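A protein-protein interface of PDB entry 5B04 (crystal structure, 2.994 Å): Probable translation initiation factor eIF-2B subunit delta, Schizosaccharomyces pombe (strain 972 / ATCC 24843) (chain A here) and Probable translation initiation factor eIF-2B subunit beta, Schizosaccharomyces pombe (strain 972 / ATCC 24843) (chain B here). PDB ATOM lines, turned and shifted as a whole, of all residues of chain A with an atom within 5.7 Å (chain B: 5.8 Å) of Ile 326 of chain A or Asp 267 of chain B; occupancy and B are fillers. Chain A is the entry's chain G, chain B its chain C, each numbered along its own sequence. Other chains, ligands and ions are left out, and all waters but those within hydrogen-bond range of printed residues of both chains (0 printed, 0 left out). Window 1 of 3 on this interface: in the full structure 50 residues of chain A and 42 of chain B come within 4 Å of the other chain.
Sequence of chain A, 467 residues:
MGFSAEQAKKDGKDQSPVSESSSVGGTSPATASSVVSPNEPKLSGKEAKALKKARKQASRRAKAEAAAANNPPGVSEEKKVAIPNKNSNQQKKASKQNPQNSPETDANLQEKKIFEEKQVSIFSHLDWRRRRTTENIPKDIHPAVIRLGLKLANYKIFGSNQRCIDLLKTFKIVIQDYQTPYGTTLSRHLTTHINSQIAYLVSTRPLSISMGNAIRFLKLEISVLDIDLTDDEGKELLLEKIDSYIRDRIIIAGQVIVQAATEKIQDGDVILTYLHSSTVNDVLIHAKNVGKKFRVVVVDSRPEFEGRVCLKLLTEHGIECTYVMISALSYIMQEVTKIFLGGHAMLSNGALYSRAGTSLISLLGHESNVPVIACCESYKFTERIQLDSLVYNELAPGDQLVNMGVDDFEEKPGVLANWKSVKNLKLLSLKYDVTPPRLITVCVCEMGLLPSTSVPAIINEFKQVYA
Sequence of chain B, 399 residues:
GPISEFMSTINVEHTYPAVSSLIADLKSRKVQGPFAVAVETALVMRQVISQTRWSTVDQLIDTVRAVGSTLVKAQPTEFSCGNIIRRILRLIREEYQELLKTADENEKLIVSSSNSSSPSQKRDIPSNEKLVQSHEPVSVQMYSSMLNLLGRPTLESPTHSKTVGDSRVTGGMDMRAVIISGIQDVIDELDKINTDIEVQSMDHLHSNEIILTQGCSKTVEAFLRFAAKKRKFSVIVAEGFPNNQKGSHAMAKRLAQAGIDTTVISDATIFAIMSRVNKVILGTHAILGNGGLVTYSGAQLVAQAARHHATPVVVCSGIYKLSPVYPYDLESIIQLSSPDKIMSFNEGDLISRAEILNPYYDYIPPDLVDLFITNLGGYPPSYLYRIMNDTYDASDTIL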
ATOM      1  N   TYR A 274      20.298  19.577 -15.984  1.00  0.00           N
ATOM      2  CA  TYR A 274      20.575  20.773 -16.734  1.00  0.00           C
ATOM      3  C   TYR A 274      19.254  21.257 -17.281  1.00  0.00           C
ATOM      4  O   TYR A 274      18.460  20.500 -17.750  1.00  0.00           O
ATOM      5  CB  TYR A 274      21.679  20.466 -17.722  1.00  0.00           C
ATOM      6  CG  TYR A 274      21.968  21.522 -18.732  1.00  0.00           C
ATOM      7  CD1 TYR A 274      22.190  22.818 -18.371  1.00  0.00           C
ATOM      8  CD2 TYR A 274      22.043  21.211 -20.037  1.00  0.00           C
ATOM      9  CE1 TYR A 274      22.461  23.773 -19.308  1.00  0.00           C
ATOM     10  CE2 TYR A 274      22.304  22.159 -20.971  1.00  0.00           C
ATOM     11  CZ  TYR A 274      22.513  23.431 -20.596  1.00  0.00           C
ATOM     12  OH  TYR A 274      22.784  24.344 -21.549  1.00  0.00           O
ATOM     13  N   VAL A 299      21.850  23.312 -13.328  1.00  0.00           N
ATOM     14  CA  VAL A 299      22.721  24.121 -14.170  1.00  0.00           C
ATOM     15  C   VAL A 299      21.903  24.847 -15.231  1.00  0.00           C
ATOM     16  O   VAL A 299      21.176  24.219 -16.001  1.00  0.00           O
ATOM     17  CB  VAL A 299      23.805  23.265 -14.851  1.00  0.00           C
ATOM     18  CG1 VAL A 299      24.622  24.108 -15.813  1.00  0.00           C
ATOM     19  CG2 VAL A 299      24.703  22.619 -13.807  1.00  0.00           C
ATOM     20  N   ASP A 300      22.021  26.169 -15.264  1.00  0.00           N
ATOM     21  CA  ASP A 300      21.253  26.981 -16.199  1.00  0.00           C
ATOM     22  C   ASP A 300      22.155  27.579 -17.273  1.00  0.00           C
ATOM     23  O   ASP A 300      23.378  27.449 -17.207  1.00  0.00           O
ATOM     24  CB  ASP A 300      20.511  28.091 -15.454  1.00  0.00           C
ATOM     25  CG  ASP A 300      19.198  28.459 -16.113  1.00  0.00           C
ATOM     26  OD1 ASP A 300      19.009  28.120 -17.301  1.00  0.00           O
ATOM     27  OD2 ASP A 300      18.351  29.083 -15.439  1.00  0.00           O
ATOM     28  N   SER A 301      21.550  28.233 -18.260  1.00  0.00           N
ATOM     29  CA  SER A 301      22.308  28.862 -19.337  1.00  0.00           C
ATOM     30  C   SER A 301      21.531  29.991 -20.009  1.00  0.00           C
ATOM     31  O   SER A 301      20.309  30.076 -19.892  1.00  0.00           O
ATOM     32  CB  SER A 301      22.713  27.820 -20.380  1.00  0.00           C
ATOM     33  OG  SER A 301      23.436  28.423 -21.440  1.00  0.00           O
ATOM     34  N   VAL A 324      23.480  27.109 -10.305  1.00  0.00           N
ATOM     35  CA  VAL A 324      24.652  27.740 -10.907  1.00  0.00           C
ATOM     36  C   VAL A 324      24.486  27.888 -12.415  1.00  0.00           C
ATOM     37  O   VAL A 324      23.680  27.190 -13.030  1.00  0.00           O
ATOM     38  CB  VAL A 324      25.944  26.937 -10.634  1.00  0.00           C
ATOM     39  CG1 VAL A 324      26.260  26.904  -9.144  1.00  0.00           C
ATOM     40  CG2 VAL A 324      25.824  25.528 -11.194  1.00  0.00           C
ATOM     41  N   MET A 325      25.253  28.797 -13.010  1.00  0.00           N
ATOM     42  CA  MET A 325      25.282  28.925 -14.463  1.00  0.00           C
ATOM     43  C   MET A 325      26.267  27.920 -15.047  1.00  0.00           C
ATOM     44  O   MET A 325      27.131  27.403 -14.337  1.00  0.00           O
ATOM     45  CB  MET A 325      25.658  30.345 -14.886  1.00  0.00           C
ATOM     46  CG  MET A 325      24.654  31.406 -14.475  1.00  0.00           C
ATOM     47  SD  MET A 325      22.972  31.013 -14.984  1.00  0.00           S
ATOM     48  CE  MET A 325      23.139  31.084 -16.759  1.00  0.00           C
ATOM     49  N   ILE A 326      26.140  27.655 -16.344  1.00  0.00           N
ATOM     50  CA  ILE A 326      26.969  26.657 -17.014  1.00  0.00           C
ATOM     51  C   ILE A 326      28.451  27.045 -16.985  1.00  0.00           C
ATOM     52  O   ILE A 326      29.328  26.201 -17.165  1.00  0.00           O
ATOM     53  CB  ILE A 326      26.509  26.444 -18.478  1.00  0.00           C
ATOM     54  CG1 ILE A 326      27.106  25.158 -19.057  1.00  0.00           C
ATOM     55  CG2 ILE A 326      26.847  27.655 -19.336  1.00  0.00           C
ATOM     56  CD1 ILE A 326      26.557  24.787 -20.416  1.00  0.00           C
ATOM     57  N   SER A 327      28.723  28.323 -16.736  1.00  0.00           N
ATOM     58  CA  SER A 327      30.093  28.809 -16.631  1.00  0.00           C
ATOM     59  C   SER A 327      30.770  28.281 -15.371  1.00  0.00           C
ATOM     60  O   SER A 327      31.996  28.199 -15.300  1.00  0.00           O
ATOM     61  CB  SER A 327      30.120  30.336 -16.631  1.00  0.00           C
ATOM     62  OG  SER A 327      29.337  30.860 -17.689  1.00  0.00           O
ATOM     63  N   ALA A 328      29.961  27.927 -14.377  1.00  0.00           N
ATOM     64  CA  ALA A 328      30.473  27.444 -13.101  1.00  0.00           C
ATOM     65  C   ALA A 328      30.442  25.924 -13.033  1.00  0.00           C
ATOM     66  O   ALA A 328      30.451  25.344 -11.947  1.00  0.00           O
ATOM     67  CB  ALA A 328      29.674  28.038 -11.952  1.00  0.00           C
ATOM     68  N   LEU A 329      30.411  25.284 -14.199  1.00  0.00           N
ATOM     69  CA  LEU A 329      30.286  23.834 -14.281  1.00  0.00           C
ATOM     70  C   LEU A 329      31.444  23.114 -13.596  1.00  0.00           C
ATOM     71  O   LEU A 329      31.227  22.215 -12.786  1.00  0.00           O
ATOM     72  CB  LEU A 329      30.191  23.388 -15.739  1.00  0.00           C
ATOM     73  CG  LEU A 329      29.872  21.907 -15.938  1.00  0.00           C
ATOM     74  CD1 LEU A 329      28.564  21.551 -15.248  1.00  0.00           C
ATOM     75  CD2 LEU A 329      29.814  21.565 -17.417  1.00  0.00           C
ATOM     76  N   SER A 330      32.668  23.514 -13.929  1.00  0.00           N
ATOM     77  CA  SER A 330      33.869  22.915 -13.351  1.00  0.00           C
ATOM     78  C   SER A 330      33.864  22.974 -11.831  1.00  0.00           C
ATOM     79  O   SER A 330      34.232  22.011 -11.158  1.00  0.00           O
ATOM     80  CB  SER A 330      35.117  23.615 -13.882  1.00  0.00           C
ATOM     81  OG  SER A 330      36.291  23.069 -13.305  1.00  0.00           O
ATOM     82  N   GLY A 357      23.879  22.975 -24.322  1.00  0.00           N
ATOM     83  CA  GLY A 357      24.988  22.861 -23.390  1.00  0.00           C
ATOM     84  C   GLY A 357      25.213  21.470 -22.826  1.00  0.00           C
ATOM     85  O   GLY A 357      26.111  21.261 -22.008  1.00  0.00           O
ATOM     86  N   THR A 358      24.408  20.516 -23.280  1.00  0.00           N
ATOM     87  CA  THR A 358      24.383  19.174 -22.703  1.00  0.00           C
ATOM     88  C   THR A 358      25.711  18.421 -22.839  1.00  0.00           C
ATOM     89  O   THR A 358      26.115  17.702 -21.924  1.00  0.00           O
ATOM     90  CB  THR A 358      23.262  18.332 -23.338  1.00  0.00           C
ATOM     91  OG1 THR A 358      22.029  19.061 -23.282  1.00  0.00           O
ATOM     92  CG2 THR A 358      23.097  17.013 -22.603  1.00  0.00           C
ATOM     93  N   LEU A 360      28.696  19.689 -22.902  1.00  0.00           N
ATOM     94  CA  LEU A 360      29.623  20.262 -21.934  1.00  0.00           C
ATOM     95  C   LEU A 360      29.385  19.668 -20.552  1.00  0.00           C
ATOM     96  O   LEU A 360      30.331  19.407 -19.807  1.00  0.00           O
ATOM     97  CB  LEU A 360      29.487  21.785 -21.892  1.00  0.00           C
ATOM     98  CG  LEU A 360      30.136  22.537 -23.055  1.00  0.00           C
ATOM     99  CD1 LEU A 360      29.773  24.012 -23.015  1.00  0.00           C
ATOM    100  CD2 LEU A 360      31.646  22.353 -23.030  1.00  0.00           C
ATOM    101  N   ILE A 361      28.115  19.453 -20.217  1.00  0.00           N
ATOM    102  CA  ILE A 361      27.748  18.795 -18.969  1.00  0.00           C
ATOM    103  C   ILE A 361      28.354  17.399 -18.916  1.00  0.00           C
ATOM    104  O   ILE A 361      28.974  17.012 -17.925  1.00  0.00           O
ATOM    105  CB  ILE A 361      26.217  18.686 -18.807  1.00  0.00           C
ATOM    106  CG1 ILE A 361      25.561  20.066 -18.886  1.00  0.00           C
ATOM    107  CG2 ILE A 361      25.865  17.995 -17.499  1.00  0.00           C
ATOM    108  CD1 ILE A 361      25.852  20.952 -17.697  1.00  0.00           C
ATOM    109  N   GLN B 214      37.148  33.669 -25.279  1.00  0.00           N
ATOM    110  CA  GLN B 214      36.096  33.842 -24.290  1.00  0.00           C
ATOM    111  C   GLN B 214      36.351  35.066 -23.421  1.00  0.00           C
ATOM    112  O   GLN B 214      37.498  35.405 -23.131  1.00  0.00           O
ATOM    113  CB  GLN B 214      35.973  32.596 -23.412  1.00  0.00           C
ATOM    114  CG  GLN B 214      34.690  32.544 -22.605  1.00  0.00           C
ATOM    115  CD  GLN B 214      34.787  31.605 -21.425  1.00  0.00           C
ATOM    116  OE1 GLN B 214      33.835  30.893 -21.105  1.00  0.00           O
ATOM    117  NE2 GLN B 214      35.937  31.607 -20.763  1.00  0.00           N
ATOM    118  N   ALA B 238      32.926  33.845 -27.065  1.00  0.00           N
ATOM    119  CA  ALA B 238      32.021  33.335 -26.049  1.00  0.00           C
ATOM    120  C   ALA B 238      31.914  34.355 -24.924  1.00  0.00           C
ATOM    121  O   ALA B 238      32.919  34.713 -24.309  1.00  0.00           O
ATOM    122  CB  ALA B 238      32.504  31.995 -25.519  1.00  0.00           C
ATOM    123  N   GLU B 239      30.701  34.837 -24.674  1.00  0.00           N
ATOM    124  CA  GLU B 239      30.461  35.761 -23.573  1.00  0.00           C
ATOM    125  C   GLU B 239      30.885  35.112 -22.262  1.00  0.00           C
ATOM    126  O   GLU B 239      30.743  33.905 -22.090  1.00  0.00           O
ATOM    127  CB  GLU B 239      28.989  36.171 -23.514  1.00  0.00           C
ATOM    128  CG  GLU B 239      28.037  34.996 -23.389  1.00  0.00           C
ATOM    129  CD  GLU B 239      26.642  35.411 -22.976  1.00  0.00           C
ATOM    130  OE1 GLU B 239      26.204  36.513 -23.366  1.00  0.00           O
ATOM    131  OE2 GLU B 239      25.986  34.632 -22.256  1.00  0.00           O
ATOM    132  N   GLY B 240      31.418  35.908 -21.344  1.00  0.00           N
ATOM    133  CA  GLY B 240      31.880  35.378 -20.076  1.00  0.00           C
ATOM    134  C   GLY B 240      30.812  35.462 -19.005  1.00  0.00           C
ATOM    135  O   GLY B 240      31.078  35.907 -17.889  1.00  0.00           O
ATOM    136  N   PHE B 241      29.603  35.029 -19.348  1.00  0.00           N
ATOM    137  CA  PHE B 241      28.467  35.133 -18.441  1.00  0.00           C
ATOM    138  C   PHE B 241      28.709  34.375 -17.139  1.00  0.00           C
ATOM    139  O   PHE B 241      29.182  33.242 -17.161  1.00  0.00           O
ATOM    140  CB  PHE B 241      27.196  34.615 -19.112  1.00  0.00           C
ATOM    141  CG  PHE B 241      25.956  34.916 -18.337  1.00  0.00           C
ATOM    142  CD1 PHE B 241      25.374  36.162 -18.415  1.00  0.00           C
ATOM    143  CD2 PHE B 241      25.394  33.971 -17.499  1.00  0.00           C
ATOM    144  CE1 PHE B 241      24.250  36.449 -17.692  1.00  0.00           C
ATOM    145  CE2 PHE B 241      24.260  34.265 -16.772  1.00  0.00           C
ATOM    146  CZ  PHE B 241      23.687  35.506 -16.871  1.00  0.00           C
ATOM    147  N   ILE B 265      28.511  34.115 -29.178  1.00  0.00           N
ATOM    148  CA  ILE B 265      27.775  32.926 -28.763  1.00  0.00           C
ATOM    149  C   ILE B 265      27.619  32.841 -27.249  1.00  0.00           C
ATOM    150  O   ILE B 265      28.406  33.417 -26.498  1.00  0.00           O
ATOM    151  CB  ILE B 265      28.465  31.632 -29.249  1.00  0.00           C
ATOM    152  CG1 ILE B 265      29.827  31.467 -28.570  1.00  0.00           C
ATOM    153  CG2 ILE B 265      28.610  31.636 -30.762  1.00  0.00           C
ATOM    154  CD1 ILE B 265      30.446  30.101 -28.762  1.00  0.00           C
ATOM    155  N   SER B 266      26.596  32.116 -26.810  1.00  0.00           N
ATOM    156  CA  SER B 266      26.438  31.799 -25.398  1.00  0.00           C
ATOM    157  C   SER B 266      27.471  30.750 -25.002  1.00  0.00           C
ATOM    158  O   SER B 266      28.065  30.103 -25.865  1.00  0.00           O
ATOM    159  CB  SER B 266      25.021  31.301 -25.107  1.00  0.00           C
ATOM    160  OG  SER B 266      24.673  30.223 -25.958  1.00  0.00           O
ATOM    161  N   ASP B 267      27.688  30.582 -23.703  1.00  0.00           N
ATOM    162  CA  ASP B 267      28.700  29.647 -23.217  1.00  0.00           C
ATOM    163  C   ASP B 267      28.329  28.195 -23.497  1.00  0.00           C
ATOM    164  O   ASP B 267      29.199  27.328 -23.567  1.00  0.00           O
ATOM    165  CB  ASP B 267      28.930  29.840 -21.719  1.00  0.00           C
ATOM    166  CG  ASP B 267      29.607  31.154 -21.400  1.00  0.00           C
ATOM    167  OD1 ASP B 267      30.850  31.219 -21.505  1.00  0.00           O
ATOM    168  OD2 ASP B 267      28.896  32.117 -21.045  1.00  0.00           O
ATOM    169  N   ALA B 268      27.036  27.933 -23.653  1.00  0.00           N
ATOM    170  CA  ALA B 268      26.563  26.579 -23.918  1.00  0.00           C
ATOM    171  C   ALA B 268      26.931  26.132 -25.328  1.00  0.00           C
ATOM    172  O   ALA B 268      27.059  24.939 -25.599  1.00  0.00           O
ATOM    173  CB  ALA B 268      25.061  26.496 -23.711  1.00  0.00           C
ATOM    174  N   THR B 269      27.111  27.100 -26.221  1.00  0.00           N
ATOM    175  CA  THR B 269      27.345  26.817 -27.632  1.00  0.00           C
ATOM    176  C   THR B 269      28.810  26.478 -27.923  1.00  0.00           C
ATOM    177  O   THR B 269      29.153  26.091 -29.040  1.00  0.00           O
ATOM    178  CB  THR B 269      26.921  28.017 -28.507  1.00  0.00           C
ATOM    179  OG1 THR B 269      25.775  28.650 -27.926  1.00  0.00           O
ATOM    180  CG2 THR B 269      26.581  27.567 -29.923  1.00  0.00           C
ATOM    181  N   ILE B 270      29.662  26.612 -26.910  1.00  0.00           N
ATOM    182  CA  ILE B 270      31.105  26.423 -27.070  1.00  0.00           C
ATOM    183  C   ILE B 270      31.476  25.074 -27.687  1.00  0.00           C
ATOM    184  O   ILE B 270      32.240  25.018 -28.652  1.00  0.00           O
ATOM    185  CB  ILE B 270      31.833  26.567 -25.718  1.00  0.00           C
ATOM    186  CG1 ILE B 270      31.801  28.024 -25.256  1.00  0.00           C
ATOM    187  CG2 ILE B 270      33.274  26.090 -25.829  1.00  0.00           C
ATOM    188  CD1 ILE B 270      32.408  28.245 -23.893  1.00  0.00           C
ATOM    189  N   PHE B 271      30.931  23.993 -27.139  1.00  0.00           N
ATOM    190  CA  PHE B 271      31.224  22.654 -27.641  1.00  0.00           C
ATOM    191  C   PHE B 271      30.715  22.472 -29.068  1.00  0.00           C
ATOM    192  O   PHE B 271      31.378  21.846 -29.897  1.00  0.00           O
ATOM    193  CB  PHE B 271      30.606  21.592 -26.727  1.00  0.00           C
ATOM    194  CG  PHE B 271      31.029  20.181 -27.051  1.00  0.00           C
ATOM    195  CD1 PHE B 271      30.388  19.456 -28.045  1.00  0.00           C
ATOM    196  CD2 PHE B 271      32.059  19.577 -26.350  1.00  0.00           C
ATOM    197  CE1 PHE B 271      30.773  18.163 -28.338  1.00  0.00           C
ATOM    198  CE2 PHE B 271      32.448  18.281 -26.638  1.00  0.00           C
ATOM    199  CZ  PHE B 271      31.803  17.574 -27.634  1.00  0.00           C
ATOM    200  N   SER B 297      35.795  32.676 -15.114  1.00  0.00           N
ATOM    201  CA  SER B 297      34.884  31.533 -15.163  1.00  0.00           C
ATOM    202  C   SER B 297      34.382  31.210 -16.566  1.00  0.00           C
ATOM    203  O   SER B 297      34.117  32.107 -17.368  1.00  0.00           O
ATOM    204  CB  SER B 297      33.688  31.772 -14.238  1.00  0.00           C
ATOM    205  OG  SER B 297      32.833  32.774 -14.759  1.00  0.00           O
ATOM    206  N   GLY B 298      34.259  29.918 -16.849  1.00  0.00           N
ATOM    207  CA  GLY B 298      33.785  29.453 -18.139  1.00  0.00           C
ATOM    208  C   GLY B 298      34.912  28.969 -19.029  1.00  0.00           C
ATOM    209  O   GLY B 298      34.675  28.300 -20.034  1.00  0.00           O
ATOM    210  N   LEU B 301      35.240  25.261 -19.710  1.00  0.00           N
ATOM    211  CA  LEU B 301      34.388  24.786 -20.794  1.00  0.00           C
ATOM    212  C   LEU B 301      35.155  24.797 -22.107  1.00  0.00           C
ATOM    213  O   LEU B 301      35.150  23.817 -22.849  1.00  0.00           O
ATOM    214  CB  LEU B 301      33.129  25.646 -20.917  1.00  0.00           C
ATOM    215  CG  LEU B 301      32.188  25.698 -19.714  1.00  0.00           C
ATOM    216  CD1 LEU B 301      30.969  26.550 -20.034  1.00  0.00           C
ATOM    217  CD2 LEU B 301      31.773  24.297 -19.290  1.00  0.00           C
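The side-chain hydroxyl (OG) of Ser 327 of chain A sits at hydrogen-bond distance from the backbone carbonyl oxygen (O) of Phe 241 of chain B (2.4 Å). The backbone NH (N) of Gly 298 of chain B lies within hydrogen-bond range of the backbone carbonyl oxygen (O) of Ser 327 of chain A.
The side-chain carboxylate of Asp 267 of chain B sits at hydrogen-bond distance from the backbone NH of Phe 241 of chain B (3.4 Å). The side-chain hydroxyl (OH) of Tyr 274 of chain A sits close to the backbone NH (N) of Gly 357 of chain A. The side-chain amide oxygen (OE1) of Gln 214 of chain B sits close to the side-chain carboxylate (OD1) of Asp 267 of chain B (3.0 Å). O of Asp 300 of chain A lies within hydrogen-bond range of N of Ile 326 of chain A (2.9 Å). The backbone carbonyl oxygen (O) of Gly 298 of chain B lies close to the side-chain amide oxygen (OE1) of Gln 214 of chain B (2.9 Å).
Among the printed residues, pairs that only touch across the chains: Tyr 274 of chain A with Ala 268 of chain B (3.8 Å), Ser 301 of chain A with Ala 268 of chain B (3.4 Å), Met 325 of chain A with Phe 241 of chain B (3.4 Å), Ile 326 of chain A with Asp 267 of chain B (3.8 Å), Ile 326 of chain A with Ala 268 of chain B (3.9 Å), Ile 326 of chain A with Leu 301 of chain B (3.3 Å), Ser 327 of chain A with Asp 267 of chain B (3.6 Å), Leu 329 of chain A with Leu 301 of chain B (3.8 Å), Gly 357 of chain A with Ala 268 of chain B (3.6 Å), Leu 360 of chain A with Asp 267 of chain B (3.4 Å), Leu 360 of chain A with Ala 268 of chain B (3.9 Å), Leu 360 of chain A with Phe 271 of chain B (3.8 Å) and Leu 360 of chain A with Leu 301 of chain B (3.8 Å).
Of chain B, only Asp 267, Ala 268 and Leu 301 come within 4 Å of Ile 326 of chain A. Asp 267 of chain B touches just these residues of chain A: Ile 326 (3.8 Å), Ser 327 (3.6 Å) and Leu 360 (3.4 Å). Of the printed residues of chain B, Ser 301 of chain A touches Ala 268 (3.4 Å). Printed residues of chain A within 4 Å of Phe 271 of chain B: Leu 360 (3.8 Å). Glu 239 of chain B touches none of the printed residues of chain A. The nearest residue of chain B that does not touch Ile 326 of chain A is Gly 298 of chain B (5.6 Å). The nearest residue of chain A that does not touch Asp 267 of chain B is Ser 301 of chain A (5.3 Å).
Hydrophobic or aromatic side chains of chain A that line the printed part of chain B: Tyr 274, Met 325, Ile 326, Leu 329 and Leu 360. Hydrophobic or aromatic side chains of chain B within 4 Å of the printed part of chain A: Phe 241, Ala 268, Phe 271 and Leu 301. Among the printed residues, no Asp or Glu carboxylate lies within 4 Å of a Lys or Arg side-chain nitrogen of the other chain.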
